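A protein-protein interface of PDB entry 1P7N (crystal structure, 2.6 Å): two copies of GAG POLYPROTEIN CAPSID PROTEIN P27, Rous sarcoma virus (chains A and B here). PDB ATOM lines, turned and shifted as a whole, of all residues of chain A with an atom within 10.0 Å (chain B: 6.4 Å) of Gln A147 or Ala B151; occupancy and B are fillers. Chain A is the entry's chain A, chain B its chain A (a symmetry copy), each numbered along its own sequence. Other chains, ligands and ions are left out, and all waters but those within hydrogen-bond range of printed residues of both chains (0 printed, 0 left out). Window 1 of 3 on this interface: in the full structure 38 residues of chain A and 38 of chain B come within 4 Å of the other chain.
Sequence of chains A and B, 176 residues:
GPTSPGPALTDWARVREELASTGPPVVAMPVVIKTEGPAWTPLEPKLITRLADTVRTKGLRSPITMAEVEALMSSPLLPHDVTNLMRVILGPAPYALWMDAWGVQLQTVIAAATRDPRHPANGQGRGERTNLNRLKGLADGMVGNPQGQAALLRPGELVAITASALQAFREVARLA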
ATOM      1  N   ALA A   8      16.154 -15.065 -15.006  1.00  0.00           N
ATOM      2  CA  ALA A   8      15.660 -14.294 -13.865  1.00  0.00           C
ATOM      3  C   ALA A   8      15.543 -15.265 -12.702  1.00  0.00           C
ATOM      4  O   ALA A   8      16.098 -15.046 -11.628  1.00  0.00           O
ATOM      5  CB  ALA A   8      14.306 -13.692 -14.174  1.00  0.00           C
ATOM      6  N   LEU A   9      14.823 -16.351 -12.933  1.00  0.00           N
ATOM      7  CA  LEU A   9      14.646 -17.376 -11.922  1.00  0.00           C
ATOM      8  C   LEU A   9      15.577 -18.507 -12.318  1.00  0.00           C
ATOM      9  O   LEU A   9      15.611 -18.908 -13.475  1.00  0.00           O
ATOM     10  CB  LEU A   9      13.196 -17.856 -11.914  1.00  0.00           C
ATOM     11  CG  LEU A   9      12.314 -17.552 -10.694  1.00  0.00           C
ATOM     12  CD1 LEU A   9      12.550 -16.158 -10.145  1.00  0.00           C
ATOM     13  CD2 LEU A   9      10.859 -17.733 -11.117  1.00  0.00           C
ATOM     14  N   TRP A  40      -1.172 -11.962 -17.284  1.00  0.00           N
ATOM     15  CA  TRP A  40      -1.631 -10.585 -17.205  1.00  0.00           C
ATOM     16  C   TRP A  40      -0.864  -9.770 -18.240  1.00  0.00           C
ATOM     17  O   TRP A  40       0.143 -10.224 -18.763  1.00  0.00           O
ATOM     18  CB  TRP A  40      -1.407 -10.003 -15.800  1.00  0.00           C
ATOM     19  CG  TRP A  40      -0.059 -10.277 -15.281  1.00  0.00           C
ATOM     20  CD1 TRP A  40       0.368 -11.435 -14.696  1.00  0.00           C
ATOM     21  CD2 TRP A  40       1.091  -9.433 -15.386  1.00  0.00           C
ATOM     22  NE1 TRP A  40       1.711 -11.369 -14.440  1.00  0.00           N
ATOM     23  CE2 TRP A  40       2.183 -10.149 -14.853  1.00  0.00           C
ATOM     24  CE3 TRP A  40       1.306  -8.147 -15.885  1.00  0.00           C
ATOM     25  CZ2 TRP A  40       3.478  -9.619 -14.802  1.00  0.00           C
ATOM     26  CZ3 TRP A  40       2.601  -7.619 -15.838  1.00  0.00           C
ATOM     27  CH2 TRP A  40       3.667  -8.359 -15.298  1.00  0.00           C
ATOM     28  N   LEU A  78      -3.885  -7.040 -13.610  1.00  0.00           N
ATOM     29  CA  LEU A  78      -3.743  -7.284 -12.181  1.00  0.00           C
ATOM     30  C   LEU A  78      -4.656  -6.299 -11.445  1.00  0.00           C
ATOM     31  O   LEU A  78      -4.953  -5.217 -11.949  1.00  0.00           O
ATOM     32  CB  LEU A  78      -2.286  -7.072 -11.752  1.00  0.00           C
ATOM     33  CG  LEU A  78      -1.212  -7.957 -12.398  1.00  0.00           C
ATOM     34  CD1 LEU A  78       0.178  -7.444 -12.018  1.00  0.00           C
ATOM     35  CD2 LEU A  78      -1.400  -9.408 -11.967  1.00  0.00           C
ATOM     36  N   PRO A  79      -5.127  -6.668 -10.248  1.00  0.00           N
ATOM     37  CA  PRO A  79      -6.008  -5.794  -9.459  1.00  0.00           C
ATOM     38  C   PRO A  79      -5.418  -4.395  -9.342  1.00  0.00           C
ATOM     39  O   PRO A  79      -6.135  -3.385  -9.376  1.00  0.00           O
ATOM     40  CB  PRO A  79      -6.057  -6.484  -8.097  1.00  0.00           C
ATOM     41  CG  PRO A  79      -5.878  -7.930  -8.439  1.00  0.00           C
ATOM     42  CD  PRO A  79      -4.808  -7.907  -9.510  1.00  0.00           C
ATOM     43  N   HIS A  80      -4.099  -4.349  -9.205  1.00  0.00           N
ATOM     44  CA  HIS A  80      -3.382  -3.095  -9.051  1.00  0.00           C
ATOM     45  C   HIS A  80      -3.588  -2.218 -10.248  1.00  0.00           C
ATOM     46  O   HIS A  80      -3.797  -1.018 -10.128  1.00  0.00           O
ATOM     47  CB  HIS A  80      -1.889  -3.360  -8.878  1.00  0.00           C
ATOM     48  CG  HIS A  80      -1.095  -2.126  -8.587  1.00  0.00           C
ATOM     49  ND1 HIS A  80      -1.211  -1.428  -7.403  1.00  0.00           N
ATOM     50  CD2 HIS A  80      -0.208  -1.435  -9.344  1.00  0.00           C
ATOM     51  CE1 HIS A  80      -0.434  -0.362  -7.445  1.00  0.00           C
ATOM     52  NE2 HIS A  80       0.185  -0.342  -8.612  1.00  0.00           N
ATOM     53  N   ASP A  81      -3.526  -2.841 -11.418  1.00  0.00           N
ATOM     54  CA  ASP A  81      -3.675  -2.149 -12.672  1.00  0.00           C
ATOM     55  C   ASP A  81      -5.080  -1.657 -12.929  1.00  0.00           C
ATOM     56  O   ASP A  81      -5.264  -0.499 -13.298  1.00  0.00           O
ATOM     57  CB  ASP A  81      -3.230  -3.053 -13.811  1.00  0.00           C
ATOM     58  CG  ASP A  81      -1.718  -3.141 -13.934  1.00  0.00           C
ATOM     59  OD1 ASP A  81      -1.000  -2.389 -13.222  1.00  0.00           O
ATOM     60  OD2 ASP A  81      -1.259  -3.968 -14.763  1.00  0.00           O
ATOM     61  N   GLY A 137      -6.884  -8.016  -4.893  1.00  0.00           N
ATOM     62  CA  GLY A 137      -5.471  -7.757  -4.662  1.00  0.00           C
ATOM     63  C   GLY A 137      -5.273  -7.236  -3.249  1.00  0.00           C
ATOM     64  O   GLY A 137      -4.405  -6.404  -2.973  1.00  0.00           O
ATOM     65  N   ASP A 140      -3.316 -11.294   1.433  1.00  0.00           N
ATOM     66  CA  ASP A 140      -2.016 -11.083   2.057  1.00  0.00           C
ATOM     67  C   ASP A 140      -0.887 -11.281   1.070  1.00  0.00           C
ATOM     68  O   ASP A 140      -0.776 -12.339   0.436  1.00  0.00           O
ATOM     69  CB  ASP A 140      -1.843 -12.032   3.244  1.00  0.00           C
ATOM     70  CG  ASP A 140      -0.692 -11.627   4.141  1.00  0.00           C
ATOM     71  OD1 ASP A 140      -0.746 -10.501   4.694  1.00  0.00           O
ATOM     72  OD2 ASP A 140       0.261 -12.429   4.290  1.00  0.00           O
ATOM     73  N   GLY A 141      -0.043 -10.261   0.942  1.00  0.00           N
ATOM     74  CA  GLY A 141       1.059 -10.351   0.003  1.00  0.00           C
ATOM     75  C   GLY A 141       0.745  -9.669  -1.317  1.00  0.00           C
ATOM     76  O   GLY A 141       1.628  -9.486  -2.157  1.00  0.00           O
ATOM     77  N   MET A 142      -0.515  -9.295  -1.504  1.00  0.00           N
ATOM     78  CA  MET A 142      -0.935  -8.611  -2.710  1.00  0.00           C
ATOM     79  C   MET A 142      -1.093  -7.128  -2.422  1.00  0.00           C
ATOM     80  O   MET A 142      -0.810  -6.282  -3.262  1.00  0.00           O
ATOM     81  CB  MET A 142      -2.250  -9.181  -3.190  1.00  0.00           C
ATOM     82  CG  MET A 142      -2.144 -10.595  -3.635  1.00  0.00           C
ATOM     83  SD  MET A 142      -3.714 -11.110  -4.224  1.00  0.00           S
ATOM     84  CE  MET A 142      -3.478 -12.912  -4.224  1.00  0.00           C
ATOM     85  N   VAL A 143      -1.570  -6.823  -1.225  1.00  0.00           N
ATOM     86  CA  VAL A 143      -1.740  -5.447  -0.793  1.00  0.00           C
ATOM     87  C   VAL A 143      -0.500  -4.625  -1.134  1.00  0.00           C
ATOM     88  O   VAL A 143       0.595  -4.899  -0.622  1.00  0.00           O
ATOM     89  CB  VAL A 143      -1.973  -5.394   0.721  1.00  0.00           C
ATOM     90  CG1 VAL A 143      -3.447  -5.589   1.038  1.00  0.00           C
ATOM     91  CG2 VAL A 143      -1.168  -6.519   1.384  1.00  0.00           C
ATOM     92  N   GLY A 144      -0.685  -3.632  -2.006  1.00  0.00           N
ATOM     93  CA  GLY A 144       0.398  -2.752  -2.419  1.00  0.00           C
ATOM     94  C   GLY A 144       1.580  -3.476  -3.021  1.00  0.00           C
ATOM     95  O   GLY A 144       2.689  -2.939  -3.075  1.00  0.00           O
ATOM     96  N   ASN A 145       1.335  -4.690  -3.509  1.00  0.00           N
ATOM     97  CA  ASN A 145       2.388  -5.525  -4.080  1.00  0.00           C
ATOM     98  C   ASN A 145       1.984  -6.117  -5.439  1.00  0.00           C
ATOM     99  O   ASN A 145       1.621  -7.295  -5.536  1.00  0.00           O
ATOM    100  CB  ASN A 145       2.698  -6.634  -3.067  1.00  0.00           C
ATOM    101  CG  ASN A 145       3.908  -7.455  -3.438  1.00  0.00           C
ATOM    102  OD1 ASN A 145       4.641  -7.130  -4.367  1.00  0.00           O
ATOM    103  ND2 ASN A 145       4.132  -8.534  -2.694  1.00  0.00           N
ATOM    104  N   PRO A 146       2.039  -5.307  -6.510  1.00  0.00           N
ATOM    105  CA  PRO A 146       1.666  -5.799  -7.850  1.00  0.00           C
ATOM    106  C   PRO A 146       2.500  -7.002  -8.275  1.00  0.00           C
ATOM    107  O   PRO A 146       2.019  -7.897  -8.969  1.00  0.00           O
ATOM    108  CB  PRO A 146       1.876  -4.584  -8.743  1.00  0.00           C
ATOM    109  CG  PRO A 146       2.903  -3.766  -8.005  1.00  0.00           C
ATOM    110  CD  PRO A 146       2.501  -3.909  -6.565  1.00  0.00           C
ATOM    111  N   GLN A 147       3.755  -7.003  -7.835  1.00  0.00           N
ATOM    112  CA  GLN A 147       4.722  -8.068  -8.084  1.00  0.00           C
ATOM    113  C   GLN A 147       4.138  -9.309  -7.411  1.00  0.00           C
ATOM    114  O   GLN A 147       4.133 -10.413  -7.970  1.00  0.00           O
ATOM    115  CB  GLN A 147       6.040  -7.656  -7.429  1.00  0.00           C
ATOM    116  CG  GLN A 147       7.066  -8.738  -7.200  1.00  0.00           C
ATOM    117  CD  GLN A 147       7.960  -8.973  -8.396  1.00  0.00           C
ATOM    118  OE1 GLN A 147       8.942  -9.723  -8.308  1.00  0.00           O
ATOM    119  NE2 GLN A 147       7.626  -8.345  -9.530  1.00  0.00           N
ATOM    120  N   GLY A 148       3.621  -9.099  -6.203  1.00  0.00           N
ATOM    121  CA  GLY A 148       3.016 -10.179  -5.458  1.00  0.00           C
ATOM    122  C   GLY A 148       1.801 -10.702  -6.177  1.00  0.00           C
ATOM    123  O   GLY A 148       1.619 -11.910  -6.272  1.00  0.00           O
ATOM    124  N   GLN A 149       0.967  -9.802  -6.691  1.00  0.00           N
ATOM    125  CA  GLN A 149      -0.243 -10.197  -7.429  1.00  0.00           C
ATOM    126  C   GLN A 149       0.050 -11.016  -8.683  1.00  0.00           C
ATOM    127  O   GLN A 149      -0.635 -11.998  -8.979  1.00  0.00           O
ATOM    128  CB  GLN A 149      -1.026  -8.961  -7.819  1.00  0.00           C
ATOM    129  CG  GLN A 149      -1.586  -8.250  -6.628  1.00  0.00           C
ATOM    130  CD  GLN A 149      -2.094  -6.889  -6.980  1.00  0.00           C
ATOM    131  OE1 GLN A 149      -2.301  -6.577  -8.157  1.00  0.00           O
ATOM    132  NE2 GLN A 149      -2.306  -6.061  -5.969  1.00  0.00           N
ATOM    133  N   ALA A 150       1.074 -10.594  -9.416  1.00  0.00           N
ATOM    134  CA  ALA A 150       1.491 -11.265 -10.637  1.00  0.00           C
ATOM    135  C   ALA A 150       1.924 -12.689 -10.340  1.00  0.00           C
ATOM    136  O   ALA A 150       1.795 -13.571 -11.187  1.00  0.00           O
ATOM    137  CB  ALA A 150       2.641 -10.509 -11.276  1.00  0.00           C
ATOM    138  N   ALA A 151       2.433 -12.924  -9.135  1.00  0.00           N
ATOM    139  CA  ALA A 151       2.906 -14.258  -8.791  1.00  0.00           C
ATOM    140  C   ALA A 151       1.849 -15.150  -8.179  1.00  0.00           C
ATOM    141  O   ALA A 151       1.939 -16.374  -8.277  1.00  0.00           O
ATOM    142  CB  ALA A 151       4.085 -14.157  -7.849  1.00  0.00           C
ATOM    143  N   LEU A 152       0.833 -14.557  -7.567  1.00  0.00           N
ATOM    144  CA  LEU A 152      -0.176 -15.352  -6.897  1.00  0.00           C
ATOM    145  C   LEU A 152      -1.477 -15.571  -7.643  1.00  0.00           C
ATOM    146  O   LEU A 152      -2.042 -16.661  -7.621  1.00  0.00           O
ATOM    147  CB  LEU A 152      -0.468 -14.733  -5.531  1.00  0.00           C
ATOM    148  CG  LEU A 152       0.764 -14.561  -4.627  1.00  0.00           C
ATOM    149  CD1 LEU A 152       0.350 -14.087  -3.251  1.00  0.00           C
ATOM    150  CD2 LEU A 152       1.501 -15.879  -4.516  1.00  0.00           C
ATOM    151  N   LEU A 153      -1.964 -14.536  -8.309  1.00  0.00           N
ATOM    152  CA  LEU A 153      -3.220 -14.649  -9.017  1.00  0.00           C
ATOM    153  C   LEU A 153      -3.124 -15.610 -10.182  1.00  0.00           C
ATOM    154  O   LEU A 153      -2.128 -15.647 -10.905  1.00  0.00           O
ATOM    155  CB  LEU A 153      -3.669 -13.260  -9.470  1.00  0.00           C
ATOM    156  CG  LEU A 153      -3.818 -12.294  -8.289  1.00  0.00           C
ATOM    157  CD1 LEU A 153      -3.911 -10.877  -8.776  1.00  0.00           C
ATOM    158  CD2 LEU A 153      -5.044 -12.682  -7.472  1.00  0.00           C
ATOM    159  N   LEU A 158      -7.494 -13.513 -13.141  1.00  0.00           N
ATOM    160  CA  LEU A 158      -7.225 -12.267 -13.861  1.00  0.00           C
ATOM    161  C   LEU A 158      -8.345 -11.962 -14.851  1.00  0.00           C
ATOM    162  O   LEU A 158      -8.747 -10.812 -15.027  1.00  0.00           O
ATOM    163  CB  LEU A 158      -5.893 -12.346 -14.618  1.00  0.00           C
ATOM    164  CG  LEU A 158      -4.623 -12.526 -13.771  1.00  0.00           C
ATOM    165  CD1 LEU A 158      -3.398 -12.538 -14.689  1.00  0.00           C
ATOM    166  CD2 LEU A 158      -4.512 -11.407 -12.742  1.00  0.00           C
ATOM    167  N   LEU B   9       6.043  -4.613 -15.273  1.00  0.00           N
ATOM    168  CA  LEU B   9       4.952  -4.165 -14.427  1.00  0.00           C
ATOM    169  C   LEU B   9       4.615  -2.764 -14.900  1.00  0.00           C
ATOM    170  O   LEU B   9       5.502  -1.943 -15.095  1.00  0.00           O
ATOM    171  CB  LEU B   9       5.401  -4.143 -12.967  1.00  0.00           C
ATOM    172  CG  LEU B   9       4.774  -5.135 -11.976  1.00  0.00           C
ATOM    173  CD1 LEU B   9       4.578  -6.510 -12.583  1.00  0.00           C
ATOM    174  CD2 LEU B   9       5.683  -5.203 -10.752  1.00  0.00           C
ATOM    175  N   THR B  35       7.778  -0.978  -6.019  1.00  0.00           N
ATOM    176  CA  THR B  35       8.477  -2.004  -5.248  1.00  0.00           C
ATOM    177  C   THR B  35       9.593  -2.341  -6.228  1.00  0.00           C
ATOM    178  O   THR B  35       9.315  -2.711  -7.373  1.00  0.00           O
ATOM    179  CB  THR B  35       7.606  -3.273  -5.011  1.00  0.00           C
ATOM    180  OG1 THR B  35       6.515  -2.960  -4.131  1.00  0.00           O
ATOM    181  CG2 THR B  35       8.455  -4.399  -4.404  1.00  0.00           C
ATOM    182  N   TRP B  40      17.498 -11.071  -4.269  1.00  0.00           N
ATOM    183  CA  TRP B  40      17.989 -12.434  -4.394  1.00  0.00           C
ATOM    184  C   TRP B  40      18.804 -12.528  -5.678  1.00  0.00           C
ATOM    185  O   TRP B  40      18.731 -11.648  -6.523  1.00  0.00           O
ATOM    186  CB  TRP B  40      16.829 -13.443  -4.428  1.00  0.00           C
ATOM    187  CG  TRP B  40      15.757 -13.043  -5.350  1.00  0.00           C
ATOM    188  CD1 TRP B  40      14.759 -12.146  -5.099  1.00  0.00           C
ATOM    189  CD2 TRP B  40      15.613 -13.429  -6.720  1.00  0.00           C
ATOM    190  NE1 TRP B  40      14.010 -11.940  -6.226  1.00  0.00           N
ATOM    191  CE2 TRP B  40      14.511 -12.717  -7.239  1.00  0.00           C
ATOM    192  CE3 TRP B  40      16.311 -14.298  -7.560  1.00  0.00           C
ATOM    193  CZ2 TRP B  40      14.087 -12.849  -8.568  1.00  0.00           C
ATOM    194  CZ3 TRP B  40      15.890 -14.428  -8.888  1.00  0.00           C
ATOM    195  CH2 TRP B  40      14.787 -13.705  -9.373  1.00  0.00           C
ATOM    196  N   LEU B  78      16.722 -17.584  -2.830  1.00  0.00           N
ATOM    197  CA  LEU B  78      15.350 -17.902  -2.456  1.00  0.00           C
ATOM    198  C   LEU B  78      15.344 -19.305  -1.845  1.00  0.00           C
ATOM    199  O   LEU B  78      16.198 -20.133  -2.157  1.00  0.00           O
ATOM    200  CB  LEU B  78      14.444 -17.862  -3.693  1.00  0.00           C
ATOM    201  CG  LEU B  78      14.335 -16.537  -4.459  1.00  0.00           C
ATOM    202  CD1 LEU B  78      13.581 -16.760  -5.772  1.00  0.00           C
ATOM    203  CD2 LEU B  78      13.640 -15.489  -3.596  1.00  0.00           C
ATOM    204  N   PRO B 146       8.598 -20.320  -6.705  1.00  0.00           N
ATOM    205  CA  PRO B 146       9.786 -19.457  -6.559  1.00  0.00           C
ATOM    206  C   PRO B 146       9.493 -18.007  -6.927  1.00  0.00           C
ATOM    207  O   PRO B 146      10.050 -17.078  -6.345  1.00  0.00           O
ATOM    208  CB  PRO B 146      10.811 -20.109  -7.477  1.00  0.00           C
ATOM    209  CG  PRO B 146       9.973 -20.841  -8.492  1.00  0.00           C
ATOM    210  CD  PRO B 146       8.840 -21.398  -7.680  1.00  0.00           C
ATOM    211  N   GLN B 147       8.601 -17.841  -7.899  1.00  0.00           N
ATOM    212  CA  GLN B 147       8.138 -16.546  -8.390  1.00  0.00           C
ATOM    213  C   GLN B 147       7.450 -15.885  -7.197  1.00  0.00           C
ATOM    214  O   GLN B 147       7.640 -14.696  -6.910  1.00  0.00           O
ATOM    215  CB  GLN B 147       7.146 -16.809  -9.522  1.00  0.00           C
ATOM    216  CG  GLN B 147       6.237 -15.674  -9.923  1.00  0.00           C
ATOM    217  CD  GLN B 147       6.857 -14.749 -10.945  1.00  0.00           C
ATOM    218  OE1 GLN B 147       6.180 -13.860 -11.480  1.00  0.00           O
ATOM    219  NE2 GLN B 147       8.153 -14.938 -11.221  1.00  0.00           N
ATOM    220  N   GLY B 148       6.660 -16.691  -6.490  1.00  0.00           N
ATOM    221  CA  GLY B 148       5.961 -16.206  -5.323  1.00  0.00           C
ATOM    222  C   GLY B 148       6.938 -15.791  -4.255  1.00  0.00           C
ATOM    223  O   GLY B 148       6.766 -14.744  -3.642  1.00  0.00           O
ATOM    224  N   GLN B 149       7.968 -16.602  -4.029  1.00  0.00           N
ATOM    225  CA  GLN B 149       8.994 -16.290  -3.021  1.00  0.00           C
ATOM    226  C   GLN B 149       9.748 -14.993  -3.303  1.00  0.00           C
ATOM    227  O   GLN B 149      10.017 -14.201  -2.397  1.00  0.00           O
ATOM    228  CB  GLN B 149       9.987 -17.430  -2.939  1.00  0.00           C
ATOM    229  CG  GLN B 149       9.367 -18.680  -2.400  1.00  0.00           C
ATOM    230  CD  GLN B 149      10.249 -19.870  -2.596  1.00  0.00           C
ATOM    231  OE1 GLN B 149      11.445 -19.731  -2.870  1.00  0.00           O
ATOM    232  NE2 GLN B 149       9.676 -21.056  -2.458  1.00  0.00           N
ATOM    233  N   ALA B 150      10.090 -14.794  -4.571  1.00  0.00           N
ATOM    234  CA  ALA B 150      10.806 -13.606  -5.010  1.00  0.00           C
ATOM    235  C   ALA B 150       9.984 -12.359  -4.738  1.00  0.00           C
ATOM    236  O   ALA B 150      10.537 -11.283  -4.512  1.00  0.00           O
ATOM    237  CB  ALA B 150      11.104 -13.701  -6.494  1.00  0.00           C
ATOM    238  N   ALA B 151       8.662 -12.494  -4.751  1.00  0.00           N
ATOM    239  CA  ALA B 151       7.808 -11.334  -4.537  1.00  0.00           C
ATOM    240  C   ALA B 151       7.458 -11.083  -3.087  1.00  0.00           C
ATOM    241  O   ALA B 151       7.175  -9.948  -2.706  1.00  0.00           O
ATOM    242  CB  ALA B 151       6.537 -11.478  -5.343  1.00  0.00           C
ATOM    243  N   LEU B 152       7.495 -12.123  -2.265  1.00  0.00           N
ATOM    244  CA  LEU B 152       7.102 -11.968  -0.878  1.00  0.00           C
ATOM    245  C   LEU B 152       8.220 -11.833   0.136  1.00  0.00           C
ATOM    246  O   LEU B 152       8.133 -11.039   1.070  1.00  0.00           O
ATOM    247  CB  LEU B 152       6.195 -13.133  -0.488  1.00  0.00           C
ATOM    248  CG  LEU B 152       4.954 -13.309  -1.378  1.00  0.00           C
ATOM    249  CD1 LEU B 152       4.048 -14.385  -0.821  1.00  0.00           C
ATOM    250  CD2 LEU B 152       4.202 -11.998  -1.466  1.00  0.00           C
ATOM    251  N   LEU B 153       9.279 -12.605  -0.037  1.00  0.00           N
ATOM    252  CA  LEU B 153      10.375 -12.566   0.907  1.00  0.00           C
ATOM    253  C   LEU B 153      11.093 -11.235   0.879  1.00  0.00           C
ATOM    254  O   LEU B 153      11.311 -10.643  -0.179  1.00  0.00           O
ATOM    255  CB  LEU B 153      11.329 -13.725   0.618  1.00  0.00           C
ATOM    256  CG  LEU B 153      10.620 -15.082   0.695  1.00  0.00           C
ATOM    257  CD1 LEU B 153      11.467 -16.154   0.076  1.00  0.00           C
ATOM    258  CD2 LEU B 153      10.296 -15.400   2.149  1.00  0.00           C
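The side-chain amide nitrogen (ND2) of Asn A145 lies within hydrogen-bond range of the backbone carbonyl oxygen (O) of Ala B151 (3.4 Å).
O of Gly A141 lies within hydrogen-bond range of ND2 of Asn A145.
The side-chain amide oxygen (OD1) of Asn A145 is in hydrogen-bond range of the backbone NH (N) of Gly A148 (2.9 Å).
Trp B40 touches Ala A8.
NE2 of Gln B147 touches CD2 of Leu A9, at 3.9 Å.
CH2 of Trp A40 touches CD1 of Leu B9, at 3.4 Å.
O of Gly A141 touches CD2 of Leu B152 (3.7 Å).
Gly A144 touches Thr B35.
Asn A145 touches Leu B152.
Gln A147 touches Leu B9.
Gln A147 touches Ala B151.
CB of Ala A151 touches CG of Gln B147 (3.4 Å).
Gly B148 touches Ala A151 (CA to CB, 3.8 Å).
Gln A147 touches just these residues of chain B: Leu B9 and Ala B151.
Ala B151 touches just these residues of chain A: Asn A145, Gln A147 and Gly A148.
Of chain A, only Ala A151 comes within 4 Å of Gly B148.
No residue of chain A comes within 4 Å of Ala B150.
Leu B152 touches just these residues of chain A: Gly A141 (3.7 Å) and Asn A145 (3.7 Å).
Printed residues of chain B within 4 Å of Gly A144: Thr B35.
Printed residues of chain B within 4 Å of Gly A141: Leu B152 (3.7 Å).
Gln A149 touches none of the printed residues of chain B.
His A80 touches none of the printed residues of chain B.
The nearest residue of chain A that does not touch Ala B151 is Ala A151 (4.4 Å).
The nearest printed residue of chain B that does not touch Trp A40 is Gln B147 (5.9 Å).
Of the 12 printed residues of chain B, 7 touch a printed residue of chain A.
Of the 23 printed residues of chain A, 9 touch a printed residue of chain B.
Printed residues of chain A that touch a printed residue of chain B: Ala A8, Leu A9, Trp A40, Gly A141, Gly A144, Asn A145, Gln A147, Gly A148 and Ala A151.
Leu A9 touches Trp B40, and with the chains exchanged Trp A40 touches Leu B9.
Leu A9 touches Gln B147, and with the chains exchanged Gln A147 touches Leu B9.
Gln A147 touches Ala B151, and with the chains exchanged Ala A151 touches Gln B147.
Gly A148 touches Ala B151, and with the chains exchanged Ala A151 touches Gly B148.
Positions printed for both chains: 9, 40, 78, 146, 147, 148, 149, 150, 151, 152 and 153.
Of the 13 pairs that touch across the chains among the printed residues, 8 have their exchanged pair printed and touching as well.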
